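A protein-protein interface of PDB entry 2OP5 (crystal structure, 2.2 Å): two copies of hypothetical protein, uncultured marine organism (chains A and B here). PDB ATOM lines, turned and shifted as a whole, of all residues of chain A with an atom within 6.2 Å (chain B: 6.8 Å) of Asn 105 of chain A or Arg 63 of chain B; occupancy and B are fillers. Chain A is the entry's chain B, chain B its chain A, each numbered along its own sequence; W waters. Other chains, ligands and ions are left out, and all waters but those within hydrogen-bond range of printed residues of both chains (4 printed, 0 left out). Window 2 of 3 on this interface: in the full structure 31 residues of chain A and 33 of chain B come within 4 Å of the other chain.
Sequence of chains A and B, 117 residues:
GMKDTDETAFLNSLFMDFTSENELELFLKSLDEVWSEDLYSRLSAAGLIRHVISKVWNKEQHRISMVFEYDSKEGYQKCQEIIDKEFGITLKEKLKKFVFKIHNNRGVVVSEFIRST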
ATOM      1  N   LEU A  11     -11.487   3.770  -3.574  1.00  0.00           N
ATOM      2  CA  LEU A  11     -12.844   3.416  -3.956  1.00  0.00           C
ATOM      3  C   LEU A  11     -13.878   4.397  -3.455  1.00  0.00           C
ATOM      4  O   LEU A  11     -13.869   4.728  -2.286  1.00  0.00           O
ATOM      5  CB  LEU A  11     -13.117   2.023  -3.377  1.00  0.00           C
ATOM      6  CG  LEU A  11     -14.411   1.244  -3.647  1.00  0.00           C
ATOM      7  CD1 LEU A  11     -14.138  -0.239  -3.592  1.00  0.00           C
ATOM      8  CD2 LEU A  11     -15.519   1.565  -2.680  1.00  0.00           C
ATOM      9  N   ASN A  12     -14.735   4.891  -4.350  1.00  0.00           N
ATOM     10  CA  ASN A  12     -15.860   5.746  -3.955  1.00  0.00           C
ATOM     11  C   ASN A  12     -17.144   4.900  -4.048  1.00  0.00           C
ATOM     12  O   ASN A  12     -17.544   4.483  -5.124  1.00  0.00           O
ATOM     13  CB  ASN A  12     -15.997   7.035  -4.778  1.00  0.00           C
ATOM     14  CG  ASN A  12     -17.118   7.984  -4.228  1.00  0.00           C
ATOM     15  OD1 ASN A  12     -17.804   7.681  -3.236  1.00  0.00           O
ATOM     16  ND2 ASN A  12     -17.291   9.139  -4.881  1.00  0.00           N
ATOM     17  N   SER A  13     -17.750   4.656  -2.888  1.00  0.00           N
ATOM     18  CA  SER A  13     -19.004   3.919  -2.744  1.00  0.00           C
ATOM     19  C   SER A  13     -20.109   4.935  -2.453  1.00  0.00           C
ATOM     20  O   SER A  13     -20.447   5.270  -1.307  1.00  0.00           O
ATOM     21  CB  SER A  13     -18.857   2.849  -1.670  1.00  0.00           C
ATOM     22  OG  SER A  13     -17.935   3.288  -0.672  1.00  0.00           O
ATOM     23  N   LEU A  14     -20.687   5.381  -3.561  1.00  0.00           N
ATOM     24  CA  LEU A  14     -21.645   6.458  -3.630  1.00  0.00           C
ATOM     25  C   LEU A  14     -23.097   6.002  -3.781  1.00  0.00           C
ATOM     26  O   LEU A  14     -23.384   4.941  -4.373  1.00  0.00           O
ATOM     27  CB  LEU A  14     -21.216   7.297  -4.839  1.00  0.00           C
ATOM     28  CG  LEU A  14     -21.967   8.435  -5.481  1.00  0.00           C
ATOM     29  CD1 LEU A  14     -20.985   9.236  -6.355  1.00  0.00           C
ATOM     30  CD2 LEU A  14     -23.120   7.948  -6.320  1.00  0.00           C
ATOM     31  N   PHE A  15     -24.002   6.841  -3.263  1.00  0.00           N
ATOM     32  CA  PHE A  15     -25.444   6.598  -3.348  1.00  0.00           C
ATOM     33  C   PHE A  15     -26.177   7.805  -3.816  1.00  0.00           C
ATOM     34  O   PHE A  15     -25.917   8.892  -3.307  1.00  0.00           O
ATOM     35  CB  PHE A  15     -25.986   6.243  -1.988  1.00  0.00           C
ATOM     36  CG  PHE A  15     -25.324   5.065  -1.401  1.00  0.00           C
ATOM     37  CD1 PHE A  15     -25.615   3.807  -1.876  1.00  0.00           C
ATOM     38  CD2 PHE A  15     -24.403   5.207  -0.385  1.00  0.00           C
ATOM     39  CE1 PHE A  15     -24.999   2.706  -1.346  1.00  0.00           C
ATOM     40  CE2 PHE A  15     -23.789   4.115   0.143  1.00  0.00           C
ATOM     41  CZ  PHE A  15     -24.085   2.856  -0.340  1.00  0.00           C
ATOM     42  N   HIS A 103     -24.539  10.861  -1.815  1.00  0.00           N
ATOM     43  CA  HIS A 103     -23.792  10.494  -0.623  1.00  0.00           C
ATOM     44  C   HIS A 103     -22.538   9.796  -1.100  1.00  0.00           C
ATOM     45  O   HIS A 103     -22.609   8.712  -1.638  1.00  0.00           O
ATOM     46  CB  HIS A 103     -24.604   9.574   0.279  1.00  0.00           C
ATOM     47  CG  HIS A 103     -25.851  10.210   0.807  1.00  0.00           C
ATOM     48  ND1 HIS A 103     -25.885  10.923   1.986  1.00  0.00           N
ATOM     49  CD2 HIS A 103     -27.101  10.270   0.295  1.00  0.00           C
ATOM     50  CE1 HIS A 103     -27.110  11.375   2.185  1.00  0.00           C
ATOM     51  NE2 HIS A 103     -27.867  10.991   1.174  1.00  0.00           N
ATOM     52  N   ASN A 104     -21.401  10.447  -0.935  1.00  0.00           N
ATOM     53  CA  ASN A 104     -20.125   9.885  -1.300  1.00  0.00           C
ATOM     54  C   ASN A 104     -19.518   9.128  -0.139  1.00  0.00           C
ATOM     55  O   ASN A 104     -19.828   9.414   1.017  1.00  0.00           O
ATOM     56  CB  ASN A 104     -19.165  11.009  -1.667  1.00  0.00           C
ATOM     57  CG  ASN A 104     -19.560  11.723  -2.918  1.00  0.00           C
ATOM     58  OD1 ASN A 104     -19.420  11.187  -4.019  1.00  0.00           O
ATOM     59  ND2 ASN A 104     -20.015  12.967  -2.772  1.00  0.00           N
ATOM     60  N   ASN A 105     -18.643   8.176  -0.459  1.00  0.00           N
ATOM     61  CA  ASN A 105     -17.884   7.413   0.533  1.00  0.00           C
ATOM     62  C   ASN A 105     -16.563   7.055  -0.085  1.00  0.00           C
ATOM     63  O   ASN A 105     -16.406   5.989  -0.693  1.00  0.00           O
ATOM     64  CB  ASN A 105     -18.614   6.164   0.976  1.00  0.00           C
ATOM     65  CG  ASN A 105     -19.816   6.477   1.836  1.00  0.00           C
ATOM     66  OD1 ASN A 105     -19.681   6.962   2.958  1.00  0.00           O
ATOM     67  ND2 ASN A 105     -20.994   6.240   1.301  1.00  0.00           N
ATOM     68  N   ARG A 106     -15.633   7.990   0.085  1.00  0.00           N
ATOM     69  CA  ARG A 106     -14.305   7.957  -0.507  1.00  0.00           C
ATOM     70  C   ARG A 106     -13.346   7.328   0.490  1.00  0.00           C
ATOM     71  O   ARG A 106     -13.258   7.752   1.632  1.00  0.00           O
ATOM     72  CB  ARG A 106     -13.863   9.391  -0.830  1.00  0.00           C
ATOM     73  CG  ARG A 106     -14.915  10.223  -1.598  1.00  0.00           C
ATOM     74  CD  ARG A 106     -14.474  11.677  -1.692  1.00  0.00           C
ATOM     75  NE  ARG A 106     -15.484  12.595  -2.232  1.00  0.00           N
ATOM     76  CZ  ARG A 106     -15.889  12.641  -3.504  1.00  0.00           C
ATOM     77  NH1 ARG A 106     -15.426  11.784  -4.406  1.00  0.00           N
ATOM     78  NH2 ARG A 106     -16.798  13.535  -3.883  1.00  0.00           N
ATOM     79  N   GLY A 107     -12.646   6.293   0.069  1.00  0.00           N
ATOM     80  CA  GLY A 107     -11.747   5.643   0.984  1.00  0.00           C
ATOM     81  C   GLY A 107     -10.634   4.839   0.372  1.00  0.00           C
ATOM     82  O   GLY A 107     -10.680   4.432  -0.807  1.00  0.00           O
ATOM     83  N   SER B  13     -23.443  -2.937  -0.922  1.00  0.00           N
ATOM     84  CA  SER B  13     -22.506  -1.848  -0.626  1.00  0.00           C
ATOM     85  C   SER B  13     -22.942  -1.401   0.739  1.00  0.00           C
ATOM     86  O   SER B  13     -23.878  -0.602   0.882  1.00  0.00           O
ATOM     87  CB  SER B  13     -22.622  -0.699  -1.632  1.00  0.00           C
ATOM     88  OG  SER B  13     -21.728   0.361  -1.301  1.00  0.00           O
ATOM     89  N   PHE B  15     -22.065  -0.184   4.890  1.00  0.00           N
ATOM     90  CA  PHE B  15     -21.143   0.638   5.672  1.00  0.00           C
ATOM     91  C   PHE B  15     -21.441   0.535   7.169  1.00  0.00           C
ATOM     92  O   PHE B  15     -22.571   0.227   7.567  1.00  0.00           O
ATOM     93  CB  PHE B  15     -21.020   2.101   5.159  1.00  0.00           C
ATOM     94  CG  PHE B  15     -22.280   2.955   5.285  1.00  0.00           C
ATOM     95  CD1 PHE B  15     -23.199   3.031   4.245  1.00  0.00           C
ATOM     96  CD2 PHE B  15     -22.500   3.726   6.417  1.00  0.00           C
ATOM     97  CE1 PHE B  15     -24.331   3.837   4.340  1.00  0.00           C
ATOM     98  CE2 PHE B  15     -23.644   4.531   6.530  1.00  0.00           C
ATOM     99  CZ  PHE B  15     -24.560   4.585   5.488  1.00  0.00           C
ATOM    100  N   MET B  16     -20.381   0.744   7.968  1.00  0.00           N
ATOM    101  CA  MET B  16     -20.448   0.693   9.436  1.00  0.00           C
ATOM    102  C   MET B  16     -19.791   1.927  10.026  1.00  0.00           C
ATOM    103  O   MET B  16     -18.701   2.305   9.613  1.00  0.00           O
ATOM    104  CB  MET B  16     -19.712  -0.509   9.998  1.00  0.00           C
ATOM    105  CG  MET B  16     -20.432  -1.812   9.835  1.00  0.00           C
ATOM    106  SD  MET B  16     -19.133  -3.272   9.774  1.00  0.00           S
ATOM    107  CE  MET B  16     -18.361  -2.733   8.167  1.00  0.00           C
ATOM    108  N   ASP B  17     -20.447   2.511  11.017  1.00  0.00           N
ATOM    109  CA  ASP B  17     -19.990   3.713  11.693  1.00  0.00           C
ATOM    110  C   ASP B  17     -19.743   3.392  13.151  1.00  0.00           C
ATOM    111  O   ASP B  17     -20.632   2.864  13.830  1.00  0.00           O
ATOM    112  CB  ASP B  17     -21.049   4.802  11.610  1.00  0.00           C
ATOM    113  CG  ASP B  17     -21.321   5.244  10.191  1.00  0.00           C
ATOM    114  OD1 ASP B  17     -20.438   5.028   9.345  1.00  0.00           O
ATOM    115  OD2 ASP B  17     -22.420   5.791   9.913  1.00  0.00           O
ATOM    116  N   PHE B  18     -18.543   3.737  13.620  1.00  0.00           N
ATOM    117  CA  PHE B  18     -18.120   3.485  14.997  1.00  0.00           C
ATOM    118  C   PHE B  18     -18.164   4.757  15.826  1.00  0.00           C
ATOM    119  O   PHE B  18     -18.144   5.871  15.280  1.00  0.00           O
ATOM    120  CB  PHE B  18     -16.719   2.848  15.000  1.00  0.00           C
ATOM    121  CG  PHE B  18     -16.676   1.513  14.306  1.00  0.00           C
ATOM    122  CD1 PHE B  18     -16.492   1.437  12.929  1.00  0.00           C
ATOM    123  CD2 PHE B  18     -16.886   0.336  15.010  1.00  0.00           C
ATOM    124  CE1 PHE B  18     -16.475   0.208  12.276  1.00  0.00           C
ATOM    125  CE2 PHE B  18     -16.881  -0.895  14.354  1.00  0.00           C
ATOM    126  CZ  PHE B  18     -16.667  -0.951  12.985  1.00  0.00           C
ATOM    127  N   GLU B  21     -12.567   6.323  16.765  1.00  0.00           N
ATOM    128  CA  GLU B  21     -11.566   5.925  15.814  1.00  0.00           C
ATOM    129  C   GLU B  21     -10.824   4.680  16.336  1.00  0.00           C
ATOM    130  O   GLU B  21     -10.582   3.750  15.575  1.00  0.00           O
ATOM    131  CB  GLU B  21     -10.598   7.078  15.544  1.00  0.00           C
ATOM    132  CG  GLU B  21      -9.647   6.838  14.382  1.00  0.00           C
ATOM    133  CD  GLU B  21     -10.349   6.694  13.029  1.00  0.00           C
ATOM    134  OE1 GLU B  21     -11.528   7.118  12.888  1.00  0.00           O
ATOM    135  OE2 GLU B  21      -9.700   6.167  12.099  1.00  0.00           O
ATOM    136  N   LEU B  24     -12.838   1.671  15.481  1.00  0.00           N
ATOM    137  CA  LEU B  24     -12.727   1.378  14.050  1.00  0.00           C
ATOM    138  C   LEU B  24     -11.408   0.667  13.748  1.00  0.00           C
ATOM    139  O   LEU B  24     -11.400  -0.356  13.053  1.00  0.00           O
ATOM    140  CB  LEU B  24     -12.860   2.672  13.230  1.00  0.00           C
ATOM    141  CG  LEU B  24     -12.635   2.649  11.706  1.00  0.00           C
ATOM    142  CD1 LEU B  24     -13.410   3.787  11.088  1.00  0.00           C
ATOM    143  CD2 LEU B  24     -11.157   2.679  11.250  1.00  0.00           C
ATOM    144  N   SER B  54     -12.779  -0.940   2.773  1.00  0.00           N
ATOM    145  CA  SER B  54     -12.240   0.384   2.653  1.00  0.00           C
ATOM    146  C   SER B  54     -12.432   1.226   3.934  1.00  0.00           C
ATOM    147  O   SER B  54     -13.373   1.037   4.685  1.00  0.00           O
ATOM    148  CB  SER B  54     -12.915   1.047   1.433  1.00  0.00           C
ATOM    149  OG  SER B  54     -12.881   2.463   1.520  1.00  0.00           O
ATOM    150  N   LYS B  55     -11.495   2.127   4.171  1.00  0.00           N
ATOM    151  CA  LYS B  55     -11.546   3.036   5.300  1.00  0.00           C
ATOM    152  C   LYS B  55     -12.014   4.347   4.691  1.00  0.00           C
ATOM    153  O   LYS B  55     -11.339   4.910   3.853  1.00  0.00           O
ATOM    154  CB  LYS B  55     -10.154   3.171   5.924  1.00  0.00           C
ATOM    155  CG  LYS B  55     -10.108   3.919   7.246  1.00  0.00           C
ATOM    156  CD  LYS B  55      -8.679   3.965   7.811  1.00  0.00           C
ATOM    157  CE  LYS B  55      -8.555   4.922   9.012  1.00  0.00           C
ATOM    158  N   VAL B  56     -13.190   4.808   5.085  1.00  0.00           N
ATOM    159  CA  VAL B  56     -13.779   6.016   4.511  1.00  0.00           C
ATOM    160  C   VAL B  56     -13.158   7.274   5.109  1.00  0.00           C
ATOM    161  O   VAL B  56     -13.008   7.375   6.319  1.00  0.00           O
ATOM    162  CB  VAL B  56     -15.324   6.005   4.672  1.00  0.00           C
ATOM    163  CG1 VAL B  56     -15.971   7.297   4.145  1.00  0.00           C
ATOM    164  CG2 VAL B  56     -15.904   4.799   3.961  1.00  0.00           C
ATOM    165  N   TRP B  57     -12.758   8.205   4.242  1.00  0.00           N
ATOM    166  CA  TRP B  57     -12.154   9.475   4.653  1.00  0.00           C
ATOM    167  C   TRP B  57     -13.297  10.470   4.816  1.00  0.00           C
ATOM    168  O   TRP B  57     -13.777  11.044   3.832  1.00  0.00           O
ATOM    169  CB  TRP B  57     -11.144   9.982   3.610  1.00  0.00           C
ATOM    170  N   ASN B  58     -13.755  10.624   6.053  1.00  0.00           N
ATOM    171  CA  ASN B  58     -14.878  11.511   6.397  1.00  0.00           C
ATOM    172  C   ASN B  58     -14.651  11.988   7.824  1.00  0.00           C
ATOM    173  O   ASN B  58     -14.662  11.187   8.753  1.00  0.00           O
ATOM    174  CB  ASN B  58     -16.210  10.760   6.277  1.00  0.00           C
ATOM    175  CG  ASN B  58     -17.430  11.639   6.567  1.00  0.00           C
ATOM    176  OD1 ASN B  58     -17.364  12.630   7.330  1.00  0.00           O
ATOM    177  ND2 ASN B  58     -18.568  11.260   5.968  1.00  0.00           N
ATOM    178  N   GLN B  61     -17.461  11.131  10.589  1.00  0.00           N
ATOM    179  CA  GLN B  61     -17.743   9.738  10.943  1.00  0.00           C
ATOM    180  C   GLN B  61     -16.474   8.911  11.176  1.00  0.00           C
ATOM    181  O   GLN B  61     -15.374   9.343  10.844  1.00  0.00           O
ATOM    182  CB  GLN B  61     -18.450   9.058   9.762  1.00  0.00           C
ATOM    183  CG  GLN B  61     -19.653   9.793   9.103  1.00  0.00           C
ATOM    184  CD  GLN B  61     -20.906   9.776   9.943  1.00  0.00           C
ATOM    185  OE1 GLN B  61     -21.057   8.926  10.832  1.00  0.00           O
ATOM    186  NE2 GLN B  61     -21.827  10.702   9.660  1.00  0.00           N
ATOM    187  N   HIS B  62     -16.638   7.721  11.752  1.00  0.00           N
ATOM    188  CA  HIS B  62     -15.557   6.731  11.847  1.00  0.00           C
ATOM    189  C   HIS B  62     -16.131   5.555  11.067  1.00  0.00           C
ATOM    190  O   HIS B  62     -16.644   4.620  11.644  1.00  0.00           O
ATOM    191  CB  HIS B  62     -15.265   6.332  13.275  1.00  0.00           C
ATOM    192  CG  HIS B  62     -14.956   7.480  14.164  1.00  0.00           C
ATOM    193  ND1 HIS B  62     -13.730   8.105  14.161  1.00  0.00           N
ATOM    194  CD2 HIS B  62     -15.694   8.089  15.120  1.00  0.00           C
ATOM    195  CE1 HIS B  62     -13.735   9.069  15.064  1.00  0.00           C
ATOM    196  NE2 HIS B  62     -14.915   9.079  15.660  1.00  0.00           N
ATOM    197  N   ARG B  63     -15.993   5.617   9.747  1.00  0.00           N
ATOM    198  CA  ARG B  63     -16.660   4.724   8.857  1.00  0.00           C
ATOM    199  C   ARG B  63     -15.798   3.722   8.070  1.00  0.00           C
ATOM    200  O   ARG B  63     -14.693   4.036   7.606  1.00  0.00           O
ATOM    201  CB  ARG B  63     -17.451   5.592   7.881  1.00  0.00           C
ATOM    202  CG  ARG B  63     -18.351   4.825   6.917  1.00  0.00           C
ATOM    203  CD  ARG B  63     -19.364   5.734   6.175  1.00  0.00           C
ATOM    204  NE  ARG B  63     -20.398   6.283   7.049  1.00  0.00           N
ATOM    205  CZ  ARG B  63     -21.393   7.063   6.638  1.00  0.00           C
ATOM    206  NH1 ARG B  63     -21.498   7.446   5.373  1.00  0.00           N
ATOM    207  NH2 ARG B  63     -22.269   7.509   7.517  1.00  0.00           N
ATOM    208  N   ILE B  64     -16.343   2.510   7.947  1.00  0.00           N
ATOM    209  CA  ILE B  64     -15.786   1.445   7.144  1.00  0.00           C
ATOM    210  C   ILE B  64     -16.826   1.101   6.093  1.00  0.00           C
ATOM    211  O   ILE B  64     -18.001   0.986   6.416  1.00  0.00           O
ATOM    212  CB  ILE B  64     -15.568   0.148   7.953  1.00  0.00           C
ATOM    213  CG1 ILE B  64     -14.537   0.356   9.059  1.00  0.00           C
ATOM    214  CG2 ILE B  64     -15.123  -0.997   7.045  1.00  0.00           C
ATOM    215  CD1 ILE B  64     -13.173   0.799   8.585  1.00  0.00           C
ATOM    216  N   SER B  65     -16.382   0.915   4.853  1.00  0.00           N
ATOM    217  CA  SER B  65     -17.252   0.434   3.767  1.00  0.00           C
ATOM    218  C   SER B  65     -16.807  -0.934   3.270  1.00  0.00           C
ATOM    219  O   SER B  65     -15.599  -1.252   3.253  1.00  0.00           O
ATOM    220  CB  SER B  65     -17.224   1.394   2.597  1.00  0.00           C
ATOM    221  OG  SER B  65     -15.944   1.473   2.034  1.00  0.00           O
ATOM    222  N   HIS B 103     -25.282  -0.411   7.734  1.00  0.00           N
ATOM    223  CA  HIS B 103     -26.174   0.131   6.717  1.00  0.00           C
ATOM    224  C   HIS B 103     -25.964  -0.655   5.454  1.00  0.00           C
ATOM    225  O   HIS B 103     -24.925  -0.518   4.822  1.00  0.00           O
ATOM    226  CB  HIS B 103     -25.883   1.594   6.471  1.00  0.00           C
ATOM    227  CG  HIS B 103     -26.346   2.467   7.585  1.00  0.00           C
ATOM    228  ND1 HIS B 103     -25.482   3.070   8.472  1.00  0.00           N
ATOM    229  CD2 HIS B 103     -27.597   2.805   7.983  1.00  0.00           C
ATOM    230  CE1 HIS B 103     -26.183   3.780   9.343  1.00  0.00           C
ATOM    231  NE2 HIS B 103     -27.468   3.622   9.078  1.00  0.00           N
HETATM  232  O   HOH W   1     -18.479   9.614   4.030  1.00  0.00           O
HETATM  233  O   HOH W   2     -15.564   3.476   0.295  1.00  0.00           O
HETATM  234  O   HOH W   3     -16.098  10.481   1.828  1.00  0.00           O
HETATM  235  O   HOH W   4     -22.274   2.327  -3.421  1.00  0.00           O
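Hydrophobic or aromatic side chains of chain B within 4 Å of the printed part of chain A: Val 56 and Trp 57.
Among the printed residues, no Asp or Glu carboxylate lies within 4 Å of a Lys or Arg side-chain nitrogen of the other chain.
N of Ser 54 of chain B lies within hydrogen-bond range of O of Ser 65 of chain B, at 2.9 Å.
O of Phe 15 of chain A lies within hydrogen-bond range of N of His 103 of chain A.
ND2 of Asn 12 of chain A sits close to NH1 of Arg 106 of chain A (3.3 Å).
The side-chain amide nitrogen of Asn 104 of chain A lies close to the guanidinium group of Arg 106 of chain A, at 3.5 Å.
The backbone NH (N) of Val 56 of chain B is in hydrogen-bond range of the backbone carbonyl oxygen (O) of Arg 63 of chain B, at 3.0 Å.
The backbone NH (N) of Asn 105 of chain A sits at hydrogen-bond distance from the side-chain amide oxygen (OD1) of Asn 12 of chain A.
The backbone NH (N) of Trp 57 of chain B is in hydrogen-bond range of the backbone carbonyl oxygen (O) of Arg 106 of chain A (2.7 Å).
The side-chain amide oxygen (OD1) of Asn 105 of chain A lies within hydrogen-bond range of the guanidinium group (NH1) of Arg 63 of chain B.
Water W1 lies within hydrogen-bond range of ND2 of Asn 58 of chain B, OD1 of Asn 105 of chain A and O of Asn 104 of chain A.
Water W2 lies within hydrogen-bond range of OG of Ser 13 of chain A (2.6 Å), OG of Ser 65 of chain B (2.7 Å), O of Asn 105 of chain A (2.8 Å), OG of Ser 54 of chain B (3.1 Å) and O of Leu 11 of chain A (3.3 Å).
Water W4 lies within hydrogen-bond range of the side-chain hydroxyl of Ser 13 of chain B and the backbone carbonyl oxygen of Leu 14 of chain A.
Water W3 lies within hydrogen-bond range of N of Arg 106 of chain A (3.1 Å) and O of Trp 57 of chain B (3.1 Å).
Of the printed residues of chain B, Asn 105 of chain A touches Val 56 (3.9 Å) and Arg 63 (3.1 Å).
Arg 63 of chain B touches just one residue of chain A: Asn 105 (3.1 Å).
Printed residues of chain B within 4 Å of Ser 13 of chain A: Ser 13 (3.8 Å) and Ser 65 (3.8 Å).
Printed residues of chain A within 4 Å of Ser 54 of chain B: Gly 107 (3.4 Å).
Of the printed residues of chain A, Ser 65 of chain B touches Ser 13.
Ile 64 of chain B touches none of the printed residues of chain A.
Glu 21 of chain B touches none of the printed residues of chain A.
The nearest printed residue of chain B that does not touch Asn 105 of chain A is Phe 15 of chain B (4.9 Å).
The nearest printed residue of chain A that does not touch Lys 55 of chain B is Arg 106 of chain A (4.1 Å).
Among the printed residues, merely in contact across the chains: Gly 107 of chain A with Lys 55 of chain B (3.0 Å), Arg 106 of chain A with Val 56 of chain B (3.4 Å), Gly 107 of chain A with Ser 54 of chain B (3.4 Å), Phe 15 of chain A with Ser 13 of chain B (3.6 Å), Ser 13 of chain A with Ser 13 of chain B (3.8 Å), Ser 13 of chain A with Ser 65 of chain B (3.8 Å) and Asn 105 of chain A with Val 56 of chain B (3.9 Å).
Ser 13 of chain B touches its own counterpart, Ser 13 of chain A.
Phe 15 of chain A touches Ser 13 of chain B, but with the chains exchanged Ser 13 of chain A does not touch Phe 15 of chain B (6.6 Å).
Of the 9 pairs that touch across the chains among the printed residues, 1 has its exchanged pair printed and touching as well.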
